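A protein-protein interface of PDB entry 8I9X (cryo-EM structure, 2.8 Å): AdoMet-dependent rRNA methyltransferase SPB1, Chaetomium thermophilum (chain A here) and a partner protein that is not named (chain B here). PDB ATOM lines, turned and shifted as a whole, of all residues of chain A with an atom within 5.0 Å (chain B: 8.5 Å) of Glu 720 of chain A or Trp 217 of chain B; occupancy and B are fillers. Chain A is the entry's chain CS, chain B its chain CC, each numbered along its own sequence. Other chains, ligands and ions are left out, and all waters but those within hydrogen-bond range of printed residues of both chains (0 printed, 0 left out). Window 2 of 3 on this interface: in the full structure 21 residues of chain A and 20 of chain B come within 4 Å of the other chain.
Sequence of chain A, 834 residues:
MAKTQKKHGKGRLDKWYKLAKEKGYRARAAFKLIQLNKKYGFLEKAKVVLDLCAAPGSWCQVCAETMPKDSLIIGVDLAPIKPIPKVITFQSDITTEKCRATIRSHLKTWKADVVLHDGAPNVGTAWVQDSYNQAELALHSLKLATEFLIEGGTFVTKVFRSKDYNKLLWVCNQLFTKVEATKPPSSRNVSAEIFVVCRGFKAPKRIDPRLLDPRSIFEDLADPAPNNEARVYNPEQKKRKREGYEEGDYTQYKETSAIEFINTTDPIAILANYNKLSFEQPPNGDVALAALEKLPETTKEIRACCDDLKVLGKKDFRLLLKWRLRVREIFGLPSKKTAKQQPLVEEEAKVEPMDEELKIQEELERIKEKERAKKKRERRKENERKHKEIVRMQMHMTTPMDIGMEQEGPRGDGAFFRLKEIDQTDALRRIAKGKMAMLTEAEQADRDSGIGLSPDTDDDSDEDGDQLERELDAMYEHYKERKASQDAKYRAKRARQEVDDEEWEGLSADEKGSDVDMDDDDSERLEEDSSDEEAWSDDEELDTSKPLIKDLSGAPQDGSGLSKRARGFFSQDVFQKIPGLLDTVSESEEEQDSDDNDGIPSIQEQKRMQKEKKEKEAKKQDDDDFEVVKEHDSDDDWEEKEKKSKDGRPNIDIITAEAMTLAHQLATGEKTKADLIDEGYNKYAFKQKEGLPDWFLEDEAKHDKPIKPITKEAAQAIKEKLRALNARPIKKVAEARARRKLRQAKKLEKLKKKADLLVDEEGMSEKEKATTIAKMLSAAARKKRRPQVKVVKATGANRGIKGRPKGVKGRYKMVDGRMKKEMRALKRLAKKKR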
ATOM      1  N   MET A 660       2.333  -3.900  12.523  1.00  0.00           N
ATOM      2  CA  MET A 660       1.636  -2.885  13.304  1.00  0.00           C
ATOM      3  C   MET A 660       2.464  -1.611  13.438  1.00  0.00           C
ATOM      4  O   MET A 660       1.900  -0.519  13.541  1.00  0.00           O
ATOM      5  CB  MET A 660       1.259  -3.437  14.677  1.00  0.00           C
ATOM      6  CG  MET A 660       0.474  -2.460  15.534  1.00  0.00           C
ATOM      7  SD  MET A 660      -1.246  -2.257  15.028  1.00  0.00           S
ATOM      8  CE  MET A 660      -1.795  -3.956  14.937  1.00  0.00           C
ATOM      9  N   GLN A 716       2.593  -3.208  22.357  1.00  0.00           N
ATOM     10  CA  GLN A 716       1.438  -3.261  23.245  1.00  0.00           C
ATOM     11  C   GLN A 716       0.151  -3.515  22.471  1.00  0.00           C
ATOM     12  O   GLN A 716      -0.722  -4.251  22.940  1.00  0.00           O
ATOM     13  CB  GLN A 716       1.336  -1.969  24.054  1.00  0.00           C
ATOM     14  CG  GLN A 716       2.454  -1.786  25.066  1.00  0.00           C
ATOM     15  CD  GLN A 716       2.451  -2.861  26.135  1.00  0.00           C
ATOM     16  OE1 GLN A 716       1.393  -3.315  26.573  1.00  0.00           O
ATOM     17  NE2 GLN A 716       3.639  -3.275  26.562  1.00  0.00           N
ATOM     18  N   ALA A 717       0.009  -2.907  21.291  1.00  0.00           N
ATOM     19  CA  ALA A 717      -1.179  -3.149  20.480  1.00  0.00           C
ATOM     20  C   ALA A 717      -1.273  -4.604  20.045  1.00  0.00           C
ATOM     21  O   ALA A 717      -2.359  -5.196  20.095  1.00  0.00           O
ATOM     22  CB  ALA A 717      -1.183  -2.227  19.263  1.00  0.00           C
ATOM     23  N   ILE A 718      -0.153  -5.199  19.630  1.00  0.00           N
ATOM     24  CA  ILE A 718      -0.163  -6.609  19.251  1.00  0.00           C
ATOM     25  C   ILE A 718      -0.510  -7.487  20.448  1.00  0.00           C
ATOM     26  O   ILE A 718      -1.312  -8.423  20.333  1.00  0.00           O
ATOM     27  CB  ILE A 718       1.185  -7.001  18.622  1.00  0.00           C
ATOM     28  CG1 ILE A 718       1.371  -6.287  17.286  1.00  0.00           C
ATOM     29  CG2 ILE A 718       1.275  -8.506  18.437  1.00  0.00           C
ATOM     30  CD1 ILE A 718       0.308  -6.629  16.273  1.00  0.00           C
ATOM     31  N   LYS A 719       0.081  -7.203  21.612  1.00  0.00           N
ATOM     32  CA  LYS A 719      -0.246  -7.980  22.803  1.00  0.00           C
ATOM     33  C   LYS A 719      -1.718  -7.872  23.176  1.00  0.00           C
ATOM     34  O   LYS A 719      -2.337  -8.888  23.513  1.00  0.00           O
ATOM     35  CB  LYS A 719       0.620  -7.543  23.983  1.00  0.00           C
ATOM     36  CG  LYS A 719       2.093  -7.863  23.824  1.00  0.00           C
ATOM     37  CD  LYS A 719       2.883  -7.450  25.054  1.00  0.00           C
ATOM     38  CE  LYS A 719       4.370  -7.699  24.861  1.00  0.00           C
ATOM     39  NZ  LYS A 719       4.684  -9.152  24.784  1.00  0.00           N
ATOM     40  N   GLU A 720      -2.292  -6.673  23.113  1.00  0.00           N
ATOM     41  CA  GLU A 720      -3.707  -6.473  23.391  1.00  0.00           C
ATOM     42  C   GLU A 720      -4.591  -7.213  22.394  1.00  0.00           C
ATOM     43  O   GLU A 720      -5.615  -7.785  22.776  1.00  0.00           O
ATOM     44  CB  GLU A 720      -4.037  -4.978  23.383  1.00  0.00           C
ATOM     45  CG  GLU A 720      -5.476  -4.655  23.742  1.00  0.00           C
ATOM     46  CD  GLU A 720      -5.750  -3.164  23.771  1.00  0.00           C
ATOM     47  OE1 GLU A 720      -4.818  -2.381  23.490  1.00  0.00           O
ATOM     48  OE2 GLU A 720      -6.897  -2.774  24.074  1.00  0.00           O
ATOM     49  N   LYS A 721      -4.213  -7.207  21.115  1.00  0.00           N
ATOM     50  CA  LYS A 721      -5.044  -7.862  20.112  1.00  0.00           C
ATOM     51  C   LYS A 721      -4.988  -9.377  20.246  1.00  0.00           C
ATOM     52  O   LYS A 721      -5.992 -10.063  20.024  1.00  0.00           O
ATOM     53  CB  LYS A 721      -4.618  -7.433  18.709  1.00  0.00           C
ATOM     54  CG  LYS A 721      -5.544  -7.947  17.625  1.00  0.00           C
ATOM     55  CD  LYS A 721      -5.451  -7.114  16.366  1.00  0.00           C
ATOM     56  CE  LYS A 721      -5.053  -7.965  15.183  1.00  0.00           C
ATOM     57  NZ  LYS A 721      -5.360  -7.296  13.890  1.00  0.00           N
ATOM     58  N   LEU A 722      -3.826  -9.922  20.610  1.00  0.00           N
ATOM     59  CA  LEU A 722      -3.665 -11.364  20.743  1.00  0.00           C
ATOM     60  C   LEU A 722      -3.927 -11.862  22.161  1.00  0.00           C
ATOM     61  O   LEU A 722      -3.763 -13.057  22.427  1.00  0.00           O
ATOM     62  CB  LEU A 722      -2.271 -11.798  20.279  1.00  0.00           C
ATOM     63  CG  LEU A 722      -2.002 -11.898  18.773  1.00  0.00           C
ATOM     64  CD1 LEU A 722      -1.923 -10.540  18.094  1.00  0.00           C
ATOM     65  CD2 LEU A 722      -0.733 -12.701  18.517  1.00  0.00           C
ATOM     66  N   ARG A 723      -4.324 -10.980  23.073  1.00  0.00           N
ATOM     67  CA  ARG A 723      -4.699 -11.413  24.413  1.00  0.00           C
ATOM     68  C   ARG A 723      -5.938 -12.298  24.347  1.00  0.00           C
ATOM     69  O   ARG A 723      -6.889 -11.998  23.620  1.00  0.00           O
ATOM     70  CB  ARG A 723      -4.966 -10.212  25.320  1.00  0.00           C
ATOM     71  CG  ARG A 723      -5.248 -10.612  26.759  1.00  0.00           C
ATOM     72  CD  ARG A 723      -5.503  -9.425  27.670  1.00  0.00           C
ATOM     73  NE  ARG A 723      -6.741  -8.732  27.337  1.00  0.00           N
ATOM     74  CZ  ARG A 723      -7.115  -7.574  27.861  1.00  0.00           C
ATOM     75  NH1 ARG A 723      -6.370  -6.948  28.757  1.00  0.00           N
ATOM     76  NH2 ARG A 723      -8.268  -7.031  27.481  1.00  0.00           N
ATOM     77  N   ASP B 209     -16.203  -4.658  19.710  1.00  0.00           N
ATOM     78  CA  ASP B 209     -14.865  -4.332  19.236  1.00  0.00           C
ATOM     79  C   ASP B 209     -13.800  -5.034  20.068  1.00  0.00           C
ATOM     80  O   ASP B 209     -12.842  -5.586  19.514  1.00  0.00           O
ATOM     81  CB  ASP B 209     -14.659  -2.820  19.263  1.00  0.00           C
ATOM     82  CG  ASP B 209     -15.330  -2.122  18.096  1.00  0.00           C
ATOM     83  OD1 ASP B 209     -15.183  -2.598  16.953  1.00  0.00           O
ATOM     84  OD2 ASP B 209     -16.004  -1.096  18.324  1.00  0.00           O
ATOM     85  N   SER B 210     -13.970  -5.044  21.390  1.00  0.00           N
ATOM     86  CA  SER B 210     -13.030  -5.736  22.263  1.00  0.00           C
ATOM     87  C   SER B 210     -13.027  -7.237  22.001  1.00  0.00           C
ATOM     88  O   SER B 210     -11.966  -7.872  22.021  1.00  0.00           O
ATOM     89  CB  SER B 210     -13.365  -5.446  23.724  1.00  0.00           C
ATOM     90  OG  SER B 210     -13.190  -4.072  24.021  1.00  0.00           O
ATOM     91  N   ILE B 211     -14.198  -7.825  21.763  1.00  0.00           N
ATOM     92  CA  ILE B 211     -14.266  -9.259  21.482  1.00  0.00           C
ATOM     93  C   ILE B 211     -13.598  -9.577  20.151  1.00  0.00           C
ATOM     94  O   ILE B 211     -12.604 -10.309  20.093  1.00  0.00           O
ATOM     95  CB  ILE B 211     -15.724  -9.751  21.505  1.00  0.00           C
ATOM     96  CG1 ILE B 211     -16.348  -9.534  22.884  1.00  0.00           C
ATOM     97  CG2 ILE B 211     -15.794 -11.218  21.119  1.00  0.00           C
ATOM     98  CD1 ILE B 211     -15.661 -10.285  23.987  1.00  0.00           C
ATOM     99  N   GLU B 212     -14.134  -9.031  19.063  1.00  0.00           N
ATOM    100  CA  GLU B 212     -13.571  -9.199  17.729  1.00  0.00           C
ATOM    101  C   GLU B 212     -13.170  -7.825  17.188  1.00  0.00           C
ATOM    102  O   GLU B 212     -13.980  -7.117  16.583  1.00  0.00           O
ATOM    103  CB  GLU B 212     -14.560  -9.933  16.820  1.00  0.00           C
ATOM    104  CG  GLU B 212     -15.919  -9.268  16.618  1.00  0.00           C
ATOM    105  CD  GLU B 212     -16.852 -10.090  15.752  1.00  0.00           C
ATOM    106  OE1 GLU B 212     -16.453 -11.195  15.327  1.00  0.00           O
ATOM    107  OE2 GLU B 212     -17.984  -9.631  15.493  1.00  0.00           O
ATOM    108  N   VAL B 213     -11.921  -7.445  17.442  1.00  0.00           N
ATOM    109  CA  VAL B 213     -11.327  -6.188  16.994  1.00  0.00           C
ATOM    110  C   VAL B 213     -11.617  -5.931  15.518  1.00  0.00           C
ATOM    111  O   VAL B 213     -11.717  -6.879  14.726  1.00  0.00           O
ATOM    112  CB  VAL B 213      -9.814  -6.176  17.265  1.00  0.00           C
ATOM    113  CG1 VAL B 213      -9.535  -6.546  18.711  1.00  0.00           C
ATOM    114  CG2 VAL B 213      -9.091  -7.127  16.327  1.00  0.00           C
ATOM    115  N   PRO B 214     -11.782  -4.676  15.115  1.00  0.00           N
ATOM    116  CA  PRO B 214     -12.017  -4.375  13.700  1.00  0.00           C
ATOM    117  C   PRO B 214     -10.802  -4.729  12.857  1.00  0.00           C
ATOM    118  O   PRO B 214      -9.684  -4.892  13.349  1.00  0.00           O
ATOM    119  CB  PRO B 214     -12.284  -2.866  13.690  1.00  0.00           C
ATOM    120  CG  PRO B 214     -12.611  -2.518  15.102  1.00  0.00           C
ATOM    121  CD  PRO B 214     -11.828  -3.465  15.947  1.00  0.00           C
ATOM    122  N   GLU B 215     -11.047  -4.854  11.552  1.00  0.00           N
ATOM    123  CA  GLU B 215      -9.993  -5.274  10.636  1.00  0.00           C
ATOM    124  C   GLU B 215      -8.846  -4.271  10.605  1.00  0.00           C
ATOM    125  O   GLU B 215      -7.674  -4.663  10.573  1.00  0.00           O
ATOM    126  CB  GLU B 215     -10.569  -5.471   9.235  1.00  0.00           C
ATOM    127  CG  GLU B 215      -9.633  -6.180   8.275  1.00  0.00           C
ATOM    128  CD  GLU B 215     -10.204  -6.273   6.875  1.00  0.00           C
ATOM    129  OE1 GLU B 215     -11.264  -5.661   6.624  1.00  0.00           O
ATOM    130  OE2 GLU B 215      -9.594  -6.954   6.025  1.00  0.00           O
ATOM    131  N   GLY B 216      -9.161  -2.979  10.618  1.00  0.00           N
ATOM    132  CA  GLY B 216      -8.140  -1.953  10.539  1.00  0.00           C
ATOM    133  C   GLY B 216      -7.753  -1.373  11.882  1.00  0.00           C
ATOM    134  O   GLY B 216      -7.232  -0.257  11.954  1.00  0.00           O
ATOM    135  N   TRP B 217      -8.009  -2.119  12.952  1.00  0.00           N
ATOM    136  CA  TRP B 217      -7.716  -1.651  14.302  1.00  0.00           C
ATOM    137  C   TRP B 217      -6.218  -1.435  14.475  1.00  0.00           C
ATOM    138  O   TRP B 217      -5.411  -2.277  14.070  1.00  0.00           O
ATOM    139  CB  TRP B 217      -8.234  -2.658  15.324  1.00  0.00           C
ATOM    140  CG  TRP B 217      -8.081  -2.220  16.741  1.00  0.00           C
ATOM    141  CD1 TRP B 217      -8.941  -1.440  17.452  1.00  0.00           C
ATOM    142  CD2 TRP B 217      -7.014  -2.557  17.632  1.00  0.00           C
ATOM    143  NE1 TRP B 217      -8.470  -1.258  18.726  1.00  0.00           N
ATOM    144  CE2 TRP B 217      -7.288  -1.936  18.863  1.00  0.00           C
ATOM    145  CE3 TRP B 217      -5.850  -3.320  17.506  1.00  0.00           C
ATOM    146  CZ2 TRP B 217      -6.443  -2.052  19.961  1.00  0.00           C
ATOM    147  CZ3 TRP B 217      -5.012  -3.432  18.597  1.00  0.00           C
ATOM    148  CH2 TRP B 217      -5.312  -2.804  19.808  1.00  0.00           C
ATOM    149  N   THR B 218      -5.847  -0.305  15.079  1.00  0.00           N
ATOM    150  CA  THR B 218      -4.453   0.022  15.334  1.00  0.00           C
ATOM    151  C   THR B 218      -4.164   0.408  16.776  1.00  0.00           C
ATOM    152  O   THR B 218      -2.990   0.492  17.147  1.00  0.00           O
ATOM    153  CB  THR B 218      -3.990   1.170  14.424  1.00  0.00           C
ATOM    154  OG1 THR B 218      -4.865   2.290  14.592  1.00  0.00           O
ATOM    155  CG2 THR B 218      -3.996   0.739  12.970  1.00  0.00           C
ATOM    156  N   GLY B 219      -5.185   0.646  17.593  1.00  0.00           N
ATOM    157  CA  GLY B 219      -4.967   1.048  18.966  1.00  0.00           C
ATOM    158  C   GLY B 219      -4.666   2.514  19.170  1.00  0.00           C
ATOM    159  O   GLY B 219      -4.278   2.900  20.278  1.00  0.00           O
ATOM    160  N   LEU B 220      -4.824   3.341  18.143  1.00  0.00           N
ATOM    161  CA  LEU B 220      -4.556   4.767  18.234  1.00  0.00           C
ATOM    162  C   LEU B 220      -5.852   5.565  18.186  1.00  0.00           C
ATOM    163  O   LEU B 220      -6.923   5.043  17.867  1.00  0.00           O
ATOM    164  CB  LEU B 220      -3.631   5.221  17.104  1.00  0.00           C
ATOM    165  CG  LEU B 220      -2.172   4.779  17.176  1.00  0.00           C
ATOM    166  CD1 LEU B 220      -1.357   5.523  16.132  1.00  0.00           C
ATOM    167  CD2 LEU B 220      -1.605   5.002  18.567  1.00  0.00           C
ATOM    168  N   PRO B 228     -11.463   6.337  17.638  1.00  0.00           N
ATOM    169  CA  PRO B 228     -10.241   5.629  17.251  1.00  0.00           C
ATOM    170  C   PRO B 228     -10.121   5.536  15.739  1.00  0.00           C
ATOM    171  O   PRO B 228     -11.102   5.320  15.026  1.00  0.00           O
ATOM    172  CB  PRO B 228     -10.412   4.244  17.886  1.00  0.00           C
ATOM    173  CG  PRO B 228     -11.878   4.116  18.134  1.00  0.00           C
ATOM    174  CD  PRO B 228     -12.346   5.496  18.463  1.00  0.00           C
ATOM    175  N   LEU B 229      -8.897   5.704  15.253  1.00  0.00           N
ATOM    176  CA  LEU B 229      -8.620   5.690  13.823  1.00  0.00           C
ATOM    177  C   LEU B 229      -8.407   4.255  13.358  1.00  0.00           C
ATOM    178  O   LEU B 229      -7.848   3.435  14.093  1.00  0.00           O
ATOM    179  CB  LEU B 229      -7.410   6.568  13.506  1.00  0.00           C
ATOM    180  CG  LEU B 229      -6.076   6.284  14.197  1.00  0.00           C
ATOM    181  CD1 LEU B 229      -5.300   5.202  13.484  1.00  0.00           C
ATOM    182  CD2 LEU B 229      -5.247   7.552  14.283  1.00  0.00           C
ATOM    183  N   ASN B 230      -8.854   3.956  12.143  1.00  0.00           N
ATOM    184  CA  ASN B 230      -8.779   2.616  11.582  1.00  0.00           C
ATOM    185  C   ASN B 230      -8.151   2.669  10.197  1.00  0.00           C
ATOM    186  O   ASN B 230      -8.283   3.666   9.483  1.00  0.00           O
ATOM    187  CB  ASN B 230     -10.167   1.977  11.499  1.00  0.00           C
ATOM    188  CG  ASN B 230     -10.600   1.355  12.808  1.00  0.00           C
ATOM    189  OD1 ASN B 230      -9.955   1.539  13.840  1.00  0.00           O
ATOM    190  ND2 ASN B 230     -11.699   0.614  12.775  1.00  0.00           N
ATOM    191  N   LEU B 231      -7.467   1.592   9.827  1.00  0.00           N
ATOM    192  CA  LEU B 231      -6.903   1.489   8.490  1.00  0.00           C
ATOM    193  C   LEU B 231      -7.975   1.061   7.496  1.00  0.00           C
ATOM    194  O   LEU B 231      -8.852   0.254   7.813  1.00  0.00           O
ATOM    195  CB  LEU B 231      -5.750   0.491   8.471  1.00  0.00           C
ATOM    196  CG  LEU B 231      -4.534   0.794   9.344  1.00  0.00           C
ATOM    197  CD1 LEU B 231      -3.586  -0.388   9.318  1.00  0.00           C
ATOM    198  CD2 LEU B 231      -3.828   2.059   8.896  1.00  0.00           C
ATOM    199  N   SER B 232      -7.900   1.607   6.288  1.00  0.00           N
ATOM    200  CA  SER B 232      -8.853   1.265   5.247  1.00  0.00           C
ATOM    201  C   SER B 232      -8.374   0.040   4.470  1.00  0.00           C
ATOM    202  O   SER B 232      -7.288  -0.499   4.704  1.00  0.00           O
ATOM    203  CB  SER B 232      -9.074   2.458   4.322  1.00  0.00           C
ATOM    204  OG  SER B 232      -7.884   2.790   3.630  1.00  0.00           O
ATOM    205  N   LEU B 236      -4.508  -1.272   4.248  1.00  0.00           N
ATOM    206  CA  LEU B 236      -4.119  -2.617   4.660  1.00  0.00           C
ATOM    207  C   LEU B 236      -3.475  -3.388   3.516  1.00  0.00           C
ATOM    208  O   LEU B 236      -2.507  -4.127   3.735  1.00  0.00           O
ATOM    209  CB  LEU B 236      -5.329  -3.377   5.200  1.00  0.00           C
ATOM    210  CG  LEU B 236      -5.853  -2.918   6.561  1.00  0.00           C
ATOM    211  CD1 LEU B 236      -7.330  -3.237   6.704  1.00  0.00           C
ATOM    212  CD2 LEU B 236      -5.053  -3.559   7.681  1.00  0.00           C
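Of the 18 printed residues of chain B, 3 touch a printed residue of chain A.
Hydrophobic or aromatic side chains of chain B within 4 Å of the printed part of chain A: Val 213 and Trp 217.
Of the 9 printed residues of chain A, 4 touch a printed residue of chain B.
Of the printed residues of chain B, Met 660 of chain A touches Thr 218 (3.9 Å).
Of the printed residues of chain B, Ala 717 of chain A touches Trp 217 and Thr 218.
Printed residues of chain B within 4 Å of Lys 721 of chain A: Val 213 (3.6 Å) and Trp 217 (3.98 Å).
Printed residues of chain A within 4 Å of Val 213 of chain B: Lys 721.
Gly 216 of chain B touches none of the printed residues of chain A.
Of the printed residues of chain A, Trp 217 of chain B touches Ala 717 (3.5 Å), Glu 720 (3.7 Å) and Lys 721 (3.98 Å).
Of the printed residues of chain A, Thr 218 of chain B touches Met 660 (3.9 Å) and Ala 717 (3.9 Å).
Leu 236 of chain B touches none of the printed residues of chain A.
The nearest residue of chain B that does not touch Glu 720 of chain A is Gly 219 of chain B (5.7 Å).
OG1 of Thr 218 of chain B lies close to O of Leu 229 of chain B.
O of Thr 218 of chain B touches SD of Met 660 of chain A, 3.9 Å away.
Trp 217 of chain B touches Ala 717 of chain A (CZ3 to O, 3.5 Å).
Ala 717 of chain A touches Thr 218 of chain B (CB to O, 3.9 Å).
CH2 of Trp 217 of chain B touches OE1 of Glu 720 of chain A, 3.7 Å away.
Lys 721 of chain A touches Val 213 of chain B (CD to CG2, 3.6 Å).
CE3 of Trp 217 of chain B touches CD of Lys 721 of chain A, 3.98 Å away.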
